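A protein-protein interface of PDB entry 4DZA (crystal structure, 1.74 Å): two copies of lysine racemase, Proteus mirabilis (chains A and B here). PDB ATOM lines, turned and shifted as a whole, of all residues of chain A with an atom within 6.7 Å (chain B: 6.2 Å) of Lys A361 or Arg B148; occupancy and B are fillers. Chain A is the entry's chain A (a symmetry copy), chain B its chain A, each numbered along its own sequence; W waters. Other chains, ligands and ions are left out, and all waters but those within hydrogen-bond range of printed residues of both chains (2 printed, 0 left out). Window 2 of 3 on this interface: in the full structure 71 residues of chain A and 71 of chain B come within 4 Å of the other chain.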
ATOM      1  N   ILE A 285     -19.113   2.928  11.357  1.00  0.00           N
ATOM      2  CA  ILE A 285     -19.486   3.807  10.228  1.00  0.00           C
ATOM      3  C   ILE A 285     -18.245   4.195   9.377  1.00  0.00           C
ATOM      4  O   ILE A 285     -17.333   4.762   9.899  1.00  0.00           O
ATOM      5  CB  ILE A 285     -20.213   5.068  10.761  1.00  0.00           C
ATOM      6  CG1 ILE A 285     -21.512   4.663  11.515  1.00  0.00           C
ATOM      7  CG2 ILE A 285     -20.551   5.988   9.597  1.00  0.00           C
ATOM      8  CD1 ILE A 285     -22.174   5.848  12.180  1.00  0.00           C
ATOM      9  N   ILE A 288     -20.177   9.353   6.556  1.00  0.00           N
ATOM     10  CA  ILE A 288     -21.490   9.986   6.822  1.00  0.00           C
ATOM     11  C   ILE A 288     -21.765  10.995   5.731  1.00  0.00           C
ATOM     12  O   ILE A 288     -20.964  11.911   5.522  1.00  0.00           O
ATOM     13  CB  ILE A 288     -21.474  10.659   8.189  1.00  0.00           C
ATOM     14  CG1 ILE A 288     -21.277   9.590   9.268  1.00  0.00           C
ATOM     15  CG2 ILE A 288     -22.752  11.449   8.385  1.00  0.00           C
ATOM     16  CD1 ILE A 288     -20.970  10.137  10.700  1.00  0.00           C
ATOM     17  N   ILE A 354     -29.398   7.889   9.183  1.00  0.00           N
ATOM     18  CA  ILE A 354     -29.101   8.440  10.514  1.00  0.00           C
ATOM     19  C   ILE A 354     -29.610   9.894  10.684  1.00  0.00           C
ATOM     20  O   ILE A 354     -29.204  10.597  11.612  1.00  0.00           O
ATOM     21  CB  ILE A 354     -27.618   8.254  10.972  1.00  0.00           C
ATOM     22  CG1 ILE A 354     -26.651   9.020  10.070  1.00  0.00           C
ATOM     23  CG2 ILE A 354     -27.249   6.733  11.068  1.00  0.00           C
ATOM     24  CD1 ILE A 354     -25.260   9.247  10.709  1.00  0.00           C
ATOM     25  N   ASN A 358     -28.179  12.535  16.130  1.00  0.00           N
ATOM     26  CA  ASN A 358     -27.152  13.550  15.968  1.00  0.00           C
ATOM     27  C   ASN A 358     -25.916  13.309  16.781  1.00  0.00           C
ATOM     28  O   ASN A 358     -25.862  12.375  17.578  1.00  0.00           O
ATOM     29  CB  ASN A 358     -27.671  14.981  16.170  1.00  0.00           C
ATOM     30  CG  ASN A 358     -28.936  15.039  16.966  1.00  0.00           C
ATOM     31  OD1 ASN A 358     -29.015  14.525  18.099  1.00  0.00           O
ATOM     32  ND2 ASN A 358     -29.958  15.665  16.384  1.00  0.00           N
ATOM     33  N   ASN A 359     -24.901  14.123  16.507  1.00  0.00           N
ATOM     34  CA  ASN A 359     -23.548  13.926  17.026  1.00  0.00           C
ATOM     35  C   ASN A 359     -22.956  12.569  16.669  1.00  0.00           C
ATOM     36  O   ASN A 359     -22.176  12.016  17.446  1.00  0.00           O
ATOM     37  CB  ASN A 359     -23.477  14.131  18.546  1.00  0.00           C
ATOM     38  CG  ASN A 359     -24.004  15.481  18.975  1.00  0.00           C
ATOM     39  OD1 ASN A 359     -23.661  16.518  18.384  1.00  0.00           O
ATOM     40  ND2 ASN A 359     -24.859  15.482  20.009  1.00  0.00           N
ATOM     41  N   ILE A 360     -23.309  12.046  15.494  1.00  0.00           N
ATOM     42  CA  ILE A 360     -22.737  10.760  15.060  1.00  0.00           C
ATOM     43  C   ILE A 360     -21.416  11.019  14.360  1.00  0.00           C
ATOM     44  O   ILE A 360     -21.268  12.043  13.683  1.00  0.00           O
ATOM     45  CB  ILE A 360     -23.714   9.963  14.149  1.00  0.00           C
ATOM     46  CG1 ILE A 360     -25.048   9.734  14.890  1.00  0.00           C
ATOM     47  CG2 ILE A 360     -23.081   8.574  13.713  1.00  0.00           C
ATOM     48  CD1 ILE A 360     -24.880   9.058  16.281  1.00  0.00           C
ATOM     49  N   LYS A 361     -20.430  10.170  14.632  1.00  0.00           N
ATOM     50  CA  LYS A 361     -19.077  10.358  14.103  1.00  0.00           C
ATOM     51  C   LYS A 361     -18.626   9.132  13.292  1.00  0.00           C
ATOM     52  O   LYS A 361     -19.000   7.992  13.588  1.00  0.00           O
ATOM     53  CB  LYS A 361     -18.061  10.643  15.240  1.00  0.00           C
ATOM     54  CG  LYS A 361     -18.283  12.011  15.980  1.00  0.00           C
ATOM     55  CD  LYS A 361     -18.020  13.196  15.032  1.00  0.00           C
ATOM     56  CE  LYS A 361     -17.856  14.559  15.752  1.00  0.00           C
ATOM     57  NZ  LYS A 361     -19.094  14.931  16.516  1.00  0.00           N
ATOM     58  N   PRO A 362     -17.841   9.367  12.238  1.00  0.00           N
ATOM     59  CA  PRO A 362     -17.153   8.258  11.601  1.00  0.00           C
ATOM     60  C   PRO A 362     -16.486   7.395  12.636  1.00  0.00           C
ATOM     61  O   PRO A 362     -15.847   7.948  13.563  1.00  0.00           O
ATOM     62  CB  PRO A 362     -16.058   8.960  10.786  1.00  0.00           C
ATOM     63  CG  PRO A 362     -16.587  10.236  10.451  1.00  0.00           C
ATOM     64  CD  PRO A 362     -17.423  10.660  11.689  1.00  0.00           C
ATOM     65  N   GLY A 363     -16.536   6.059  12.440  1.00  0.00           N
ATOM     66  CA  GLY A 363     -15.892   5.089  13.358  1.00  0.00           C
ATOM     67  C   GLY A 363     -16.783   4.665  14.503  1.00  0.00           C
ATOM     68  O   GLY A 363     -16.417   3.787  15.298  1.00  0.00           O
ATOM     69  N   ASP A 364     -17.939   5.303  14.604  1.00  0.00           N
ATOM     70  CA  ASP A 364     -18.919   4.908  15.605  1.00  0.00           C
ATOM     71  C   ASP A 364     -19.384   3.457  15.409  1.00  0.00           C
ATOM     72  O   ASP A 364     -19.612   2.986  14.272  1.00  0.00           O
ATOM     73  CB  ASP A 364     -20.124   5.854  15.633  1.00  0.00           C
ATOM     74  CG  ASP A 364     -19.865   7.151  16.500  1.00  0.00           C
ATOM     75  OD1 ASP A 364     -18.733   7.341  17.067  1.00  0.00           O
ATOM     76  OD2 ASP A 364     -20.785   7.994  16.537  1.00  0.00           O
ATOM     77  N   GLU A 365     -19.554   2.774  16.530  1.00  0.00           N
ATOM     78  CA  GLU A 365     -19.905   1.368  16.519  1.00  0.00           C
ATOM     79  C   GLU A 365     -21.340   1.118  16.080  1.00  0.00           C
ATOM     80  O   GLU A 365     -22.275   1.801  16.494  1.00  0.00           O
ATOM     81  CB  GLU A 365     -19.612   0.714  17.903  1.00  0.00           C
ATOM     82  CG  GLU A 365     -19.574  -0.864  17.898  1.00  0.00           C
ATOM     83  CD  GLU A 365     -18.826  -1.453  19.116  1.00  0.00           C
ATOM     84  OE1 GLU A 365     -19.494  -1.820  20.109  1.00  0.00           O
ATOM     85  OE2 GLU A 365     -17.579  -1.534  19.086  1.00  0.00           O
ATOM     86  N   GLU B 125     -11.301   5.223   9.396  1.00  0.00           N
ATOM     87  CA  GLU B 125      -9.969   5.718   9.736  1.00  0.00           C
ATOM     88  C   GLU B 125      -9.088   4.544  10.159  1.00  0.00           C
ATOM     89  O   GLU B 125      -7.954   4.429   9.682  1.00  0.00           O
ATOM     90  CB  GLU B 125     -10.075   6.751  10.881  1.00  0.00           C
ATOM     91  CG  GLU B 125     -10.558   8.132  10.421  1.00  0.00           C
ATOM     92  CD  GLU B 125     -11.170   8.953  11.532  1.00  0.00           C
ATOM     93  OE1 GLU B 125     -12.290   8.628  11.984  1.00  0.00           O
ATOM     94  OE2 GLU B 125     -10.513   9.918  11.979  1.00  0.00           O
ATOM     95  N   LEU B 143     -16.090  15.296   2.527  1.00  0.00           N
ATOM     96  CA  LEU B 143     -15.008  16.190   2.926  1.00  0.00           C
ATOM     97  C   LEU B 143     -14.522  15.877   4.333  1.00  0.00           C
ATOM     98  O   LEU B 143     -13.329  15.924   4.581  1.00  0.00           O
ATOM     99  CB  LEU B 143     -15.480  17.657   2.828  1.00  0.00           C
ATOM    100  CG  LEU B 143     -14.599  18.716   3.497  1.00  0.00           C
ATOM    101  CD1 LEU B 143     -13.238  18.738   2.784  1.00  0.00           C
ATOM    102  CD2 LEU B 143     -15.266  20.091   3.438  1.00  0.00           C
ATOM    103  N   ASP B 144     -15.429  15.501   5.241  1.00  0.00           N
ATOM    104  CA  ASP B 144     -14.985  15.175   6.607  1.00  0.00           C
ATOM    105  C   ASP B 144     -14.051  13.959   6.535  1.00  0.00           C
ATOM    106  O   ASP B 144     -12.977  13.923   7.199  1.00  0.00           O
ATOM    107  CB  ASP B 144     -16.174  14.858   7.529  1.00  0.00           C
ATOM    108  CG  ASP B 144     -15.725  14.676   9.020  1.00  0.00           C
ATOM    109  OD1 ASP B 144     -15.048  15.576   9.576  1.00  0.00           O
ATOM    110  OD2 ASP B 144     -15.967  13.612   9.580  1.00  0.00           O
ATOM    111  N   MET B 145     -14.431  12.961   5.729  1.00  0.00           N
ATOM    112  CA  MET B 145     -13.620  11.755   5.604  1.00  0.00           C
ATOM    113  C   MET B 145     -12.318  12.085   4.892  1.00  0.00           C
ATOM    114  O   MET B 145     -11.253  11.555   5.243  1.00  0.00           O
ATOM    115  CB  MET B 145     -14.364  10.571   4.923  1.00  0.00           C
ATOM    116  CG  MET B 145     -15.396   9.838   5.843  1.00  0.00           C
ATOM    117  SD  MET B 145     -14.771   9.395   7.473  1.00  0.00           S
ATOM    118  CE  MET B 145     -13.367   8.425   7.074  1.00  0.00           C
ATOM    119  N   ALA B 146     -12.384  13.012   3.950  1.00  0.00           N
ATOM    120  CA  ALA B 146     -11.167  13.472   3.308  1.00  0.00           C
ATOM    121  C   ALA B 146     -10.258  14.160   4.360  1.00  0.00           C
ATOM    122  O   ALA B 146      -9.074  13.850   4.424  1.00  0.00           O
ATOM    123  CB  ALA B 146     -11.463  14.399   2.185  1.00  0.00           C
ATOM    124  N   LYS B 147     -10.819  15.076   5.164  1.00  0.00           N
ATOM    125  CA  LYS B 147     -10.057  15.702   6.300  1.00  0.00           C
ATOM    126  C   LYS B 147      -9.490  14.659   7.267  1.00  0.00           C
ATOM    127  O   LYS B 147      -8.350  14.774   7.707  1.00  0.00           O
ATOM    128  CB  LYS B 147     -10.915  16.723   7.087  1.00  0.00           C
ATOM    129  CG  LYS B 147     -11.364  17.936   6.276  1.00  0.00           C
ATOM    130  CD  LYS B 147     -11.793  19.141   7.133  1.00  0.00           C
ATOM    131  CE  LYS B 147     -12.836  18.826   8.143  1.00  0.00           C
ATOM    132  NZ  LYS B 147     -13.192  20.052   8.957  1.00  0.00           N
ATOM    133  N   ARG B 148     -10.279  13.644   7.612  1.00  0.00           N
ATOM    134  CA  ARG B 148      -9.806  12.624   8.545  1.00  0.00           C
ATOM    135  C   ARG B 148      -8.679  11.775   7.953  1.00  0.00           C
ATOM    136  O   ARG B 148      -7.699  11.457   8.642  1.00  0.00           O
ATOM    137  CB  ARG B 148     -10.978  11.767   9.047  1.00  0.00           C
ATOM    138  CG  ARG B 148     -11.868  12.513   9.959  1.00  0.00           C
ATOM    139  CD  ARG B 148     -13.156  11.734  10.286  1.00  0.00           C
ATOM    140  NE  ARG B 148     -13.985  12.485  11.237  1.00  0.00           N
ATOM    141  CZ  ARG B 148     -14.017  12.255  12.540  1.00  0.00           C
ATOM    142  NH1 ARG B 148     -13.314  11.254  13.051  1.00  0.00           N
ATOM    143  NH2 ARG B 148     -14.788  13.011  13.317  1.00  0.00           N
ATOM    144  N   LEU B 149      -8.774  11.477   6.661  1.00  0.00           N
ATOM    145  CA  LEU B 149      -7.715  10.731   6.001  1.00  0.00           C
ATOM    146  C   LEU B 149      -6.476  11.608   5.895  1.00  0.00           C
ATOM    147  O   LEU B 149      -5.332  11.127   6.040  1.00  0.00           O
ATOM    148  CB  LEU B 149      -8.143  10.275   4.608  1.00  0.00           C
ATOM    149  CG  LEU B 149      -7.095   9.434   3.873  1.00  0.00           C
ATOM    150  CD1 LEU B 149      -6.638   8.222   4.716  1.00  0.00           C
ATOM    151  CD2 LEU B 149      -7.597   8.931   2.549  1.00  0.00           C
ATOM    152  N   ASP B 150      -6.698  12.879   5.626  1.00  0.00           N
ATOM    153  CA  ASP B 150      -5.576  13.792   5.499  1.00  0.00           C
ATOM    154  C   ASP B 150      -4.842  13.928   6.865  1.00  0.00           C
ATOM    155  O   ASP B 150      -3.630  13.918   6.906  1.00  0.00           O
ATOM    156  CB  ASP B 150      -6.026  15.131   4.922  1.00  0.00           C
ATOM    157  CG  ASP B 150      -4.894  16.174   4.903  1.00  0.00           C
ATOM    158  OD1 ASP B 150      -4.152  16.229   3.883  1.00  0.00           O
ATOM    159  OD2 ASP B 150      -4.808  16.941   5.889  1.00  0.00           O
ATOM    160  N   ALA B 151      -5.595  13.904   7.958  1.00  0.00           N
ATOM    161  CA  ALA B 151      -5.005  13.938   9.313  1.00  0.00           C
ATOM    162  C   ALA B 151      -4.154  12.703   9.591  1.00  0.00           C
ATOM    163  O   ALA B 151      -3.040  12.821  10.097  1.00  0.00           O
ATOM    164  CB  ALA B 151      -6.091  14.082  10.356  1.00  0.00           C
ATOM    165  N   ILE B 152      -4.642  11.531   9.155  1.00  0.00           N
ATOM    166  CA  ILE B 152      -3.909  10.268   9.223  1.00  0.00           C
ATOM    167  C   ILE B 152      -2.618  10.365   8.370  1.00  0.00           C
ATOM    168  O   ILE B 152      -1.541  10.060   8.848  1.00  0.00           O
ATOM    169  CB  ILE B 152      -4.801   9.082   8.684  1.00  0.00           C
ATOM    170  CG1 ILE B 152      -5.766   8.588   9.790  1.00  0.00           C
ATOM    171  CG2 ILE B 152      -3.914   7.945   8.120  1.00  0.00           C
ATOM    172  CD1 ILE B 152      -6.813   7.623   9.293  1.00  0.00           C
ATOM    173  N   ALA B 153      -2.713  10.849   7.140  1.00  0.00           N
ATOM    174  CA  ALA B 153      -1.506  10.988   6.334  1.00  0.00           C
ATOM    175  C   ALA B 153      -0.503  11.938   7.030  1.00  0.00           C
ATOM    176  O   ALA B 153       0.699  11.649   7.042  1.00  0.00           O
ATOM    177  CB  ALA B 153      -1.807  11.482   4.954  1.00  0.00           C
HETATM  178  O   HOH W   1     -15.097   6.166   8.972  1.00  0.00           O
HETATM  179  O   HOH W   2     -13.450   6.417  11.059  1.00  0.00           O
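The side-chain carboxylate (OE1) of Glu B125 lies within salt-bridge range of the guanidinium group (NH1) of Arg B148 (3.0 Å). The side-chain carboxylate of Asp B144 is in salt-bridge range of the guanidinium group of Arg B148 (2.8 Å). N of Lys A361 sits at hydrogen-bond distance from OD2 of Asp A364 (2.9 Å).
Among the printed residues, merely in contact across the chains: Pro A362 with Arg B148, Pro A362 with Asp B144, Pro A362 with Met B145, Lys A361 with Arg B148 and Pro A362 with Glu B125.
Ile A360 touches none of the printed residues of chain B. Lys A361 touches one residue of chain B. Of the printed residues of chain B, Pro A362 touches Glu B125 (3.95 Å), Asp B144 (3.5 Å), Met B145 (3.6 Å) and Arg B148 (3.5 Å). Printed residues of chain A within 4 Å of Glu B125: Pro A362 (3.95 Å). Of the printed residues of chain A, Asp B144 touches Pro A362. Printed residues of chain A within 4 Å of Met B145: Pro A362. Arg B148 touches two residues of chain A. The nearest printed residue of chain A that does not touch Met B145 is Ile A288 (4.9 Å).
Of the 11 printed residues of chain A, 2 touch a printed residue of chain B. Printed residues of chain A that touch a printed residue of chain B: Lys A361 and Pro A362. Hydrophobic or aromatic side chains of chain A within 4 Å of the printed part of chain B: Pro A362. Hydrophobic or aromatic side chains of chain B that line the printed part of chain A: Met B145. Among the printed residues, no Asp or Glu carboxylate lies within 4 Å of a Lys or Arg side-chain nitrogen of the other chain.
No position is printed for both chains. Of the 5 pairs that touch across the chains among the printed residues, none has its exchanged pair printed and touching as well.
Water W2 lies within hydrogen-bond range of the side-chain carboxylate of Glu B125 (2.7 Å) and the backbone NH of Gly A363 (3.4 Å). Water W1 lies within hydrogen-bond range of O of Ile A285 (2.8 Å) and SD of Met B145 (3.6 Å).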
